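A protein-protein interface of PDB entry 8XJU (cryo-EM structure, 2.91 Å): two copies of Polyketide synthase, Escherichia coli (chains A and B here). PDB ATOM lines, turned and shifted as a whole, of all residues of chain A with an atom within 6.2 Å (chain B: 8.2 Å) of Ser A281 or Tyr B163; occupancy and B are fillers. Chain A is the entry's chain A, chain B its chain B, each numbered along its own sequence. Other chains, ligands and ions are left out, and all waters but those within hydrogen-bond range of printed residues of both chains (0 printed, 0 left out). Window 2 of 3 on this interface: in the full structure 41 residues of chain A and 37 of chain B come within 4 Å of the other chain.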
ATOM      1  N   ASN A 274       7.685 -22.032 -23.067  1.00  0.00           N
ATOM      2  CA  ASN A 274       8.476 -21.922 -24.278  1.00  0.00           C
ATOM      3  C   ASN A 274       9.727 -22.762 -24.086  1.00  0.00           C
ATOM      4  O   ASN A 274      10.097 -23.110 -22.965  1.00  0.00           O
ATOM      5  CB  ASN A 274       8.801 -20.454 -24.597  1.00  0.00           C
ATOM      6  CG  ASN A 274       9.319 -20.249 -26.001  1.00  0.00           C
ATOM      7  OD1 ASN A 274      10.452 -20.576 -26.308  1.00  0.00           O
ATOM      8  ND2 ASN A 274       8.481 -19.723 -26.867  1.00  0.00           N
ATOM      9  N   GLY A 276      12.790 -21.813 -24.926  1.00  0.00           N
ATOM     10  CA  GLY A 276      13.973 -21.056 -24.632  1.00  0.00           C
ATOM     11  C   GLY A 276      15.022 -21.342 -25.686  1.00  0.00           C
ATOM     12  O   GLY A 276      14.715 -21.760 -26.799  1.00  0.00           O
ATOM     13  N   SER A 277      16.278 -21.120 -25.327  1.00  0.00           N
ATOM     14  CA  SER A 277      17.385 -21.472 -26.201  1.00  0.00           C
ATOM     15  C   SER A 277      17.944 -22.847 -25.905  1.00  0.00           C
ATOM     16  O   SER A 277      19.009 -23.192 -26.422  1.00  0.00           O
ATOM     17  CB  SER A 277      18.504 -20.437 -26.107  1.00  0.00           C
ATOM     18  OG  SER A 277      18.780 -20.109 -24.765  1.00  0.00           O
ATOM     19  N   GLU A 278      17.243 -23.645 -25.100  1.00  0.00           N
ATOM     20  CA  GLU A 278      17.712 -24.966 -24.681  1.00  0.00           C
ATOM     21  C   GLU A 278      17.352 -26.035 -25.719  1.00  0.00           C
ATOM     22  O   GLU A 278      16.691 -27.035 -25.441  1.00  0.00           O
ATOM     23  CB  GLU A 278      17.148 -25.291 -23.306  1.00  0.00           C
ATOM     24  CG  GLU A 278      17.771 -24.456 -22.202  1.00  0.00           C
ATOM     25  CD  GLU A 278      17.116 -24.657 -20.853  1.00  0.00           C
ATOM     26  OE1 GLU A 278      16.065 -25.325 -20.789  1.00  0.00           O
ATOM     27  OE2 GLU A 278      17.654 -24.142 -19.850  1.00  0.00           O
ATOM     28  N   LYS A 279      17.823 -25.797 -26.938  1.00  0.00           N
ATOM     29  CA  LYS A 279      17.614 -26.663 -28.087  1.00  0.00           C
ATOM     30  C   LYS A 279      18.699 -26.330 -29.100  1.00  0.00           C
ATOM     31  O   LYS A 279      19.497 -25.412 -28.896  1.00  0.00           O
ATOM     32  CB  LYS A 279      16.214 -26.489 -28.676  1.00  0.00           C
ATOM     33  CG  LYS A 279      15.783 -25.052 -28.833  1.00  0.00           C
ATOM     34  CD  LYS A 279      14.336 -24.967 -29.264  1.00  0.00           C
ATOM     35  CE  LYS A 279      13.954 -23.559 -29.671  1.00  0.00           C
ATOM     36  NZ  LYS A 279      12.489 -23.368 -29.806  1.00  0.00           N
ATOM     37  N   ILE A 280      18.732 -27.093 -30.193  1.00  0.00           N
ATOM     38  CA  ILE A 280      19.788 -26.925 -31.187  1.00  0.00           C
ATOM     39  C   ILE A 280      19.625 -25.605 -31.934  1.00  0.00           C
ATOM     40  O   ILE A 280      20.580 -24.834 -32.075  1.00  0.00           O
ATOM     41  CB  ILE A 280      19.808 -28.121 -32.152  1.00  0.00           C
ATOM     42  CG1 ILE A 280      19.785 -29.429 -31.364  1.00  0.00           C
ATOM     43  CG2 ILE A 280      21.045 -28.065 -33.011  1.00  0.00           C
ATOM     44  CD1 ILE A 280      19.510 -30.651 -32.201  1.00  0.00           C
ATOM     45  N   SER A 281      18.418 -25.321 -32.415  1.00  0.00           N
ATOM     46  CA  SER A 281      18.141 -24.063 -33.092  1.00  0.00           C
ATOM     47  C   SER A 281      16.689 -23.696 -32.833  1.00  0.00           C
ATOM     48  O   SER A 281      15.991 -24.363 -32.068  1.00  0.00           O
ATOM     49  CB  SER A 281      18.440 -24.144 -34.594  1.00  0.00           C
ATOM     50  OG  SER A 281      17.505 -24.950 -35.281  1.00  0.00           O
ATOM     51  N   TYR A 282      16.241 -22.622 -33.484  1.00  0.00           N
ATOM     52  CA  TYR A 282      14.898 -22.095 -33.260  1.00  0.00           C
ATOM     53  C   TYR A 282      13.819 -23.025 -33.799  1.00  0.00           C
ATOM     54  O   TYR A 282      12.725 -23.099 -33.227  1.00  0.00           O
ATOM     55  CB  TYR A 282      14.792 -20.714 -33.904  1.00  0.00           C
ATOM     56  CG  TYR A 282      13.477 -19.998 -33.714  1.00  0.00           C
ATOM     57  CD1 TYR A 282      13.103 -19.492 -32.474  1.00  0.00           C
ATOM     58  CD2 TYR A 282      12.622 -19.803 -34.783  1.00  0.00           C
ATOM     59  CE1 TYR A 282      11.909 -18.824 -32.310  1.00  0.00           C
ATOM     60  CE2 TYR A 282      11.427 -19.144 -34.627  1.00  0.00           C
ATOM     61  CZ  TYR A 282      11.079 -18.650 -33.395  1.00  0.00           C
ATOM     62  OH  TYR A 282       9.886 -17.989 -33.261  1.00  0.00           O
ATOM     63  N   THR A 283      14.105 -23.743 -34.885  1.00  0.00           N
ATOM     64  CA  THR A 283      13.154 -24.686 -35.456  1.00  0.00           C
ATOM     65  C   THR A 283      13.107 -26.018 -34.714  1.00  0.00           C
ATOM     66  O   THR A 283      12.208 -26.819 -34.976  1.00  0.00           O
ATOM     67  CB  THR A 283      13.485 -24.942 -36.925  1.00  0.00           C
ATOM     68  OG1 THR A 283      14.793 -25.515 -37.030  1.00  0.00           O
ATOM     69  CG2 THR A 283      13.453 -23.657 -37.702  1.00  0.00           C
ATOM     70  N   ALA A 284      14.047 -26.275 -33.809  1.00  0.00           N
ATOM     71  CA  ALA A 284      14.057 -27.523 -33.070  1.00  0.00           C
ATOM     72  C   ALA A 284      12.970 -27.525 -31.995  1.00  0.00           C
ATOM     73  O   ALA A 284      12.543 -26.468 -31.535  1.00  0.00           O
ATOM     74  CB  ALA A 284      15.421 -27.743 -32.424  1.00  0.00           C
ATOM     75  N   PRO A 285      12.470 -28.706 -31.616  1.00  0.00           N
ATOM     76  CA  PRO A 285      11.621 -28.805 -30.420  1.00  0.00           C
ATOM     77  C   PRO A 285      12.429 -29.195 -29.198  1.00  0.00           C
ATOM     78  O   PRO A 285      13.629 -29.448 -29.325  1.00  0.00           O
ATOM     79  CB  PRO A 285      10.621 -29.891 -30.808  1.00  0.00           C
ATOM     80  CG  PRO A 285      11.390 -30.767 -31.731  1.00  0.00           C
ATOM     81  CD  PRO A 285      12.436 -29.944 -32.411  1.00  0.00           C
ATOM     82  N   GLY A 421       7.479 -21.651 -32.880  1.00  0.00           N
ATOM     83  CA  GLY A 421       8.455 -20.824 -32.216  1.00  0.00           C
ATOM     84  C   GLY A 421       8.866 -21.296 -30.845  1.00  0.00           C
ATOM     85  O   GLY A 421       9.554 -20.554 -30.140  1.00  0.00           O
ATOM     86  N   PHE B  78      23.457 -11.766 -29.892  1.00  0.00           N
ATOM     87  CA  PHE B  78      22.473 -12.822 -29.739  1.00  0.00           C
ATOM     88  C   PHE B  78      22.791 -14.035 -30.594  1.00  0.00           C
ATOM     89  O   PHE B  78      22.059 -15.026 -30.543  1.00  0.00           O
ATOM     90  CB  PHE B  78      21.077 -12.285 -30.061  1.00  0.00           C
ATOM     91  CG  PHE B  78      20.663 -11.137 -29.200  1.00  0.00           C
ATOM     92  CD1 PHE B  78      20.172 -11.355 -27.929  1.00  0.00           C
ATOM     93  CD2 PHE B  78      20.763  -9.839 -29.659  1.00  0.00           C
ATOM     94  CE1 PHE B  78      19.798 -10.303 -27.133  1.00  0.00           C
ATOM     95  CE2 PHE B  78      20.398  -8.788 -28.868  1.00  0.00           C
ATOM     96  CZ  PHE B  78      19.909  -9.019 -27.605  1.00  0.00           C
ATOM     97  N   GLY B  79      23.884 -14.000 -31.343  1.00  0.00           N
ATOM     98  CA  GLY B  79      24.246 -15.106 -32.190  1.00  0.00           C
ATOM     99  C   GLY B  79      23.585 -15.097 -33.539  1.00  0.00           C
ATOM    100  O   GLY B  79      23.748 -16.059 -34.296  1.00  0.00           O
ATOM    101  N   ILE B  80      22.843 -14.051 -33.861  1.00  0.00           N
ATOM    102  CA  ILE B  80      22.162 -13.959 -35.140  1.00  0.00           C
ATOM    103  C   ILE B  80      23.191 -13.645 -36.210  1.00  0.00           C
ATOM    104  O   ILE B  80      23.986 -12.712 -36.066  1.00  0.00           O
ATOM    105  CB  ILE B  80      21.054 -12.896 -35.083  1.00  0.00           C
ATOM    106  CG1 ILE B  80      20.015 -13.297 -34.048  1.00  0.00           C
ATOM    107  CG2 ILE B  80      20.386 -12.740 -36.418  1.00  0.00           C
ATOM    108  CD1 ILE B  80      19.393 -12.149 -33.329  1.00  0.00           C
ATOM    109  N   GLU B  84      20.357 -13.407 -41.314  1.00  0.00           N
ATOM    110  CA  GLU B  84      19.083 -13.553 -40.631  1.00  0.00           C
ATOM    111  C   GLU B  84      18.658 -12.243 -40.000  1.00  0.00           C
ATOM    112  O   GLU B  84      17.463 -12.013 -39.827  1.00  0.00           O
ATOM    113  CB  GLU B  84      19.165 -14.624 -39.542  1.00  0.00           C
ATOM    114  CG  GLU B  84      19.913 -15.883 -39.917  1.00  0.00           C
ATOM    115  CD  GLU B  84      19.994 -16.874 -38.764  1.00  0.00           C
ATOM    116  OE1 GLU B  84      19.634 -16.504 -37.628  1.00  0.00           O
ATOM    117  OE2 GLU B  84      20.423 -18.026 -38.987  1.00  0.00           O
ATOM    118  N   LEU B  96      14.343  -7.101 -28.852  1.00  0.00           N
ATOM    119  CA  LEU B  96      15.405  -7.932 -28.274  1.00  0.00           C
ATOM    120  C   LEU B  96      16.313  -7.130 -27.370  1.00  0.00           C
ATOM    121  O   LEU B  96      16.571  -7.515 -26.221  1.00  0.00           O
ATOM    122  CB  LEU B  96      16.252  -8.587 -29.358  1.00  0.00           C
ATOM    123  CG  LEU B  96      15.930 -10.003 -29.777  1.00  0.00           C
ATOM    124  CD1 LEU B  96      16.763 -10.367 -30.954  1.00  0.00           C
ATOM    125  CD2 LEU B  96      16.228 -10.893 -28.618  1.00  0.00           C
ATOM    126  N   ALA B 111      17.932 -15.630 -18.483  1.00  0.00           N
ATOM    127  CA  ALA B 111      18.333 -16.945 -18.956  1.00  0.00           C
ATOM    128  C   ALA B 111      18.612 -17.897 -17.806  1.00  0.00           C
ATOM    129  O   ALA B 111      18.447 -19.109 -17.955  1.00  0.00           O
ATOM    130  CB  ALA B 111      19.566 -16.826 -19.842  1.00  0.00           C
ATOM    131  N   ILE B 119       7.414 -13.891 -21.543  1.00  0.00           N
ATOM    132  CA  ILE B 119       7.313 -12.728 -22.431  1.00  0.00           C
ATOM    133  C   ILE B 119       5.910 -12.602 -22.997  1.00  0.00           C
ATOM    134  O   ILE B 119       5.358 -13.561 -23.537  1.00  0.00           O
ATOM    135  CB  ILE B 119       8.390 -12.766 -23.535  1.00  0.00           C
ATOM    136  CG1 ILE B 119       8.497 -11.485 -24.406  1.00  0.00           C
ATOM    137  CG2 ILE B 119       8.560 -14.112 -24.149  1.00  0.00           C
ATOM    138  CD1 ILE B 119       8.920 -10.243 -23.850  1.00  0.00           C
ATOM    139  N   ASP B 155       8.768 -14.069 -38.625  1.00  0.00           N
ATOM    140  CA  ASP B 155       8.778 -14.753 -37.343  1.00  0.00           C
ATOM    141  C   ASP B 155       7.840 -14.068 -36.346  1.00  0.00           C
ATOM    142  O   ASP B 155       7.303 -12.985 -36.598  1.00  0.00           O
ATOM    143  CB  ASP B 155      10.210 -14.775 -36.810  1.00  0.00           C
ATOM    144  CG  ASP B 155      10.472 -15.907 -35.856  1.00  0.00           C
ATOM    145  OD1 ASP B 155       9.502 -16.571 -35.432  1.00  0.00           O
ATOM    146  OD2 ASP B 155      11.658 -16.127 -35.536  1.00  0.00           O
ATOM    147  N   SER B 156       7.638 -14.721 -35.203  1.00  0.00           N
ATOM    148  CA  SER B 156       6.913 -14.135 -34.090  1.00  0.00           C
ATOM    149  C   SER B 156       7.891 -13.446 -33.159  1.00  0.00           C
ATOM    150  O   SER B 156       8.896 -14.036 -32.772  1.00  0.00           O
ATOM    151  CB  SER B 156       6.135 -15.198 -33.319  1.00  0.00           C
ATOM    152  OG  SER B 156       5.561 -14.674 -32.136  1.00  0.00           O
ATOM    153  N   ILE B 157       7.564 -12.206 -32.782  1.00  0.00           N
ATOM    154  CA  ILE B 157       8.460 -11.363 -31.994  1.00  0.00           C
ATOM    155  C   ILE B 157       8.706 -11.953 -30.608  1.00  0.00           C
ATOM    156  O   ILE B 157       9.851 -12.042 -30.153  1.00  0.00           O
ATOM    157  CB  ILE B 157       7.907  -9.918 -31.944  1.00  0.00           C
ATOM    158  CG1 ILE B 157       8.843  -8.989 -31.195  1.00  0.00           C
ATOM    159  CG2 ILE B 157       6.461  -9.804 -31.405  1.00  0.00           C
ATOM    160  CD1 ILE B 157       8.683  -7.609 -31.628  1.00  0.00           C
ATOM    161  N   THR B 158       7.663 -12.434 -29.960  1.00  0.00           N
ATOM    162  CA  THR B 158       7.712 -12.853 -28.578  1.00  0.00           C
ATOM    163  C   THR B 158       8.480 -14.151 -28.407  1.00  0.00           C
ATOM    164  O   THR B 158       9.190 -14.317 -27.413  1.00  0.00           O
ATOM    165  CB  THR B 158       6.267 -12.940 -28.082  1.00  0.00           C
ATOM    166  OG1 THR B 158       5.676 -11.652 -28.225  1.00  0.00           O
ATOM    167  CG2 THR B 158       6.174 -13.231 -26.694  1.00  0.00           C
ATOM    168  N   THR B 159       8.454 -15.022 -29.408  1.00  0.00           N
ATOM    169  CA  THR B 159       9.285 -16.209 -29.393  1.00  0.00           C
ATOM    170  C   THR B 159      10.719 -15.961 -29.837  1.00  0.00           C
ATOM    171  O   THR B 159      11.588 -16.723 -29.426  1.00  0.00           O
ATOM    172  CB  THR B 159       8.675 -17.317 -30.257  1.00  0.00           C
ATOM    173  OG1 THR B 159       8.642 -16.902 -31.623  1.00  0.00           O
ATOM    174  CG2 THR B 159       7.287 -17.645 -29.791  1.00  0.00           C
ATOM    175  N   THR B 160      11.010 -14.926 -30.636  1.00  0.00           N
ATOM    176  CA  THR B 160      12.409 -14.537 -30.820  1.00  0.00           C
ATOM    177  C   THR B 160      13.014 -14.048 -29.516  1.00  0.00           C
ATOM    178  O   THR B 160      14.173 -14.353 -29.219  1.00  0.00           O
ATOM    179  CB  THR B 160      12.585 -13.443 -31.871  1.00  0.00           C
ATOM    180  OG1 THR B 160      11.915 -12.256 -31.452  1.00  0.00           O
ATOM    181  CG2 THR B 160      12.089 -13.870 -33.204  1.00  0.00           C
ATOM    182  N   ILE B 161      12.246 -13.286 -28.733  1.00  0.00           N
ATOM    183  CA  ILE B 161      12.719 -12.867 -27.417  1.00  0.00           C
ATOM    184  C   ILE B 161      12.927 -14.075 -26.515  1.00  0.00           C
ATOM    185  O   ILE B 161      13.965 -14.202 -25.863  1.00  0.00           O
ATOM    186  CB  ILE B 161      11.749 -11.869 -26.758  1.00  0.00           C
ATOM    187  CG1 ILE B 161      11.339 -10.723 -27.672  1.00  0.00           C
ATOM    188  CG2 ILE B 161      12.339 -11.317 -25.512  1.00  0.00           C
ATOM    189  CD1 ILE B 161      12.408  -9.992 -28.268  1.00  0.00           C
ATOM    190  N   ALA B 162      11.947 -14.983 -26.472  1.00  0.00           N
ATOM    191  CA  ALA B 162      12.046 -16.138 -25.581  1.00  0.00           C
ATOM    192  C   ALA B 162      13.134 -17.111 -26.012  1.00  0.00           C
ATOM    193  O   ALA B 162      13.715 -17.791 -25.166  1.00  0.00           O
ATOM    194  CB  ALA B 162      10.710 -16.860 -25.494  1.00  0.00           C
ATOM    195  N   TYR B 163      13.429 -17.187 -27.307  1.00  0.00           N
ATOM    196  CA  TYR B 163      14.551 -17.988 -27.767  1.00  0.00           C
ATOM    197  C   TYR B 163      15.863 -17.336 -27.384  1.00  0.00           C
ATOM    198  O   TYR B 163      16.641 -17.891 -26.609  1.00  0.00           O
ATOM    199  CB  TYR B 163      14.483 -18.185 -29.278  1.00  0.00           C
ATOM    200  CG  TYR B 163      15.633 -18.990 -29.814  1.00  0.00           C
ATOM    201  CD1 TYR B 163      15.896 -20.258 -29.327  1.00  0.00           C
ATOM    202  CD2 TYR B 163      16.457 -18.485 -30.796  1.00  0.00           C
ATOM    203  CE1 TYR B 163      16.947 -20.995 -29.799  1.00  0.00           C
ATOM    204  CE2 TYR B 163      17.512 -19.211 -31.277  1.00  0.00           C
ATOM    205  CZ  TYR B 163      17.753 -20.465 -30.773  1.00  0.00           C
ATOM    206  OH  TYR B 163      18.803 -21.202 -31.254  1.00  0.00           O
ATOM    207  N   HIS B 164      16.105 -16.122 -27.875  1.00  0.00           N
ATOM    208  CA  HIS B 164      17.396 -15.487 -27.702  1.00  0.00           C
ATOM    209  C   HIS B 164      17.680 -15.032 -26.283  1.00  0.00           C
ATOM    210  O   HIS B 164      18.807 -14.619 -26.015  1.00  0.00           O
ATOM    211  CB  HIS B 164      17.512 -14.307 -28.634  1.00  0.00           C
ATOM    212  CG  HIS B 164      17.746 -14.687 -30.050  1.00  0.00           C
ATOM    213  ND1 HIS B 164      18.800 -15.478 -30.438  1.00  0.00           N
ATOM    214  CD2 HIS B 164      17.076 -14.371 -31.178  1.00  0.00           C
ATOM    215  CE1 HIS B 164      18.765 -15.642 -31.745  1.00  0.00           C
ATOM    216  NE2 HIS B 164      17.727 -14.981 -32.219  1.00  0.00           N
ATOM    217  N   LEU B 165      16.720 -15.090 -25.368  1.00  0.00           N
ATOM    218  CA  LEU B 165      17.027 -14.743 -23.993  1.00  0.00           C
ATOM    219  C   LEU B 165      16.760 -15.887 -23.041  1.00  0.00           C
ATOM    220  O   LEU B 165      16.846 -15.678 -21.826  1.00  0.00           O
ATOM    221  CB  LEU B 165      16.223 -13.538 -23.526  1.00  0.00           C
ATOM    222  CG  LEU B 165      16.384 -12.230 -24.284  1.00  0.00           C
ATOM    223  CD1 LEU B 165      15.525 -11.256 -23.587  1.00  0.00           C
ATOM    224  CD2 LEU B 165      17.770 -11.743 -24.480  1.00  0.00           C
ATOM    225  N   ASN B 166      16.407 -17.064 -23.564  1.00  0.00           N
ATOM    226  CA  ASN B 166      16.156 -18.288 -22.799  1.00  0.00           C
ATOM    227  C   ASN B 166      15.045 -18.076 -21.778  1.00  0.00           C
ATOM    228  O   ASN B 166      15.187 -18.369 -20.590  1.00  0.00           O
ATOM    229  CB  ASN B 166      17.434 -18.801 -22.135  1.00  0.00           C
ATOM    230  CG  ASN B 166      17.332 -20.236 -21.673  1.00  0.00           C
ATOM    231  OD1 ASN B 166      16.318 -20.892 -21.853  1.00  0.00           O
ATOM    232  ND2 ASN B 166      18.379 -20.717 -21.038  1.00  0.00           N
ATOM    233  N   LEU B 167      13.937 -17.521 -22.243  1.00  0.00           N
ATOM    234  CA  LEU B 167      12.758 -17.358 -21.408  1.00  0.00           C
ATOM    235  C   LEU B 167      11.916 -18.609 -21.571  1.00  0.00           C
ATOM    236  O   LEU B 167      11.497 -18.940 -22.680  1.00  0.00           O
ATOM    237  CB  LEU B 167      11.973 -16.099 -21.783  1.00  0.00           C
ATOM    238  CG  LEU B 167      12.802 -14.853 -22.106  1.00  0.00           C
ATOM    239  CD1 LEU B 167      11.963 -13.720 -22.624  1.00  0.00           C
ATOM    240  CD2 LEU B 167      13.529 -14.425 -20.882  1.00  0.00           C
ATOM    241  N   ARG B 168      11.703 -19.323 -20.480  1.00  0.00           N
ATOM    242  CA  ARG B 168      11.072 -20.628 -20.547  1.00  0.00           C
ATOM    243  C   ARG B 168       9.659 -20.611 -19.991  1.00  0.00           C
ATOM    244  O   ARG B 168       9.161 -21.646 -19.549  1.00  0.00           O
ATOM    245  CB  ARG B 168      11.933 -21.663 -19.826  1.00  0.00           C
ATOM    246  CG  ARG B 168      13.238 -21.969 -20.542  1.00  0.00           C
ATOM    247  CD  ARG B 168      14.159 -22.788 -19.676  1.00  0.00           C
ATOM    248  NE  ARG B 168      14.284 -22.264 -18.317  1.00  0.00           N
ATOM    249  CZ  ARG B 168      15.197 -21.370 -17.939  1.00  0.00           C
ATOM    250  NH1 ARG B 168      15.250 -20.954 -16.683  1.00  0.00           N
ATOM    251  NH2 ARG B 168      16.057 -20.886 -18.820  1.00  0.00           N
ATOM    252  N   ALA B 171       5.423 -17.514 -23.957  1.00  0.00           N
ATOM    253  CA  ALA B 171       5.779 -16.488 -24.926  1.00  0.00           C
ATOM    254  C   ALA B 171       4.555 -16.180 -25.776  1.00  0.00           C
ATOM    255  O   ALA B 171       4.419 -16.670 -26.894  1.00  0.00           O
ATOM    256  CB  ALA B 171       6.942 -16.932 -25.792  1.00  0.00           C
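N of Ser A277 lies close to O of Tyr B163, at 3.5 Å. N of Ser A277 sits at hydrogen-bond distance from OD1 of Asn B166 (3.5 Å). The guanidinium group (NH2) of Arg B168 is in salt-bridge range of the side-chain carboxylate (OE2) of Glu A278, at 3.8 Å. OD1 of Asp B155 is in hydrogen-bond range of OH of Tyr A282. OH of Tyr A282 sits close to OG1 of Thr B159 (2.3 Å).
O of Tyr A282 sits at hydrogen-bond distance from NZ of Lys A279, 3.4 Å away. OG1 of Thr A283 is in hydrogen-bond range of OG of Ser A281 (3.3 Å). The side-chain amide nitrogen of Asn B166 lies within hydrogen-bond range of the backbone carbonyl oxygen of Ala B111. O of Ala B111 is in hydrogen-bond range of NH2 of Arg B168, at 3.1 Å. The backbone carbonyl oxygen of Ser B156 sits at hydrogen-bond distance from the side-chain hydroxyl of Thr B159 (3.1 Å). N of Leu B167 sits at hydrogen-bond distance from O of Ala B162, 2.9 Å away.
Among the printed residues, pairs that only touch across the chains: Gly A276 with Tyr B163 (3.2 Å), Gly A276 with Ala B162 (3.3 Å), Gly A421 with Thr B159 (3.4 Å), Asn A274 with Ala B171 (3.4 Å), Ser A281 with Tyr B163 (3.5 Å), Asn A274 with Arg B168 (3.6 Å), Asn A274 with Leu B167 (3.6 Å), Gly A276 with Asn B166 (3.6 Å), Tyr A282 with Tyr B163 (3.7 Å), Glu A278 with Asn B166 (3.7 Å), Asn A274 with Ala B162 (3.7 Å), Asn A274 with Thr B159 (3.8 Å), Gly A276 with Leu B167 (3.8 Å) and Lys A279 with Tyr B163 (3.8 Å).
Ser A281 touches just one residue of chain B: Tyr B163. Of chain A, only Gly A276 (3.2 Å), Ser A277 (3.2 Å), Lys A279 (3.8 Å), Ser A281 (3.5 Å) and Tyr A282 (3.7 Å) come within 4 Å of Tyr B163. Printed residues of chain B within 4 Å of Glu A278: Asn B166 and Arg B168. Of the printed residues of chain B, Gly A421 touches Thr B159 (3.4 Å). Of the printed residues of chain B, Lys A279 touches Tyr B163. Printed residues of chain A within 4 Å of Ala B162: Asn A274 and Gly A276. Ala A284 touches none of the printed residues of chain B. Leu B165 touches none of the printed residues of chain A. The nearest residue of chain B that does not touch Ser A281 is Glu B84 (7.8 Å). The nearest residue of chain A that does not touch Tyr B163 is Ile A280 (4.1 Å).
Of the 12 printed residues of chain A, 8 touch a printed residue of chain B. Hydrophobic or aromatic side chains of chain A within 4 Å of the printed part of chain B: Tyr A282. Among the printed residues, 19 pairs touch across the chains.
No position is printed for both chains. Of the 19 pairs that touch across the chains among the printed residues, none has its exchanged pair printed and touching as well.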
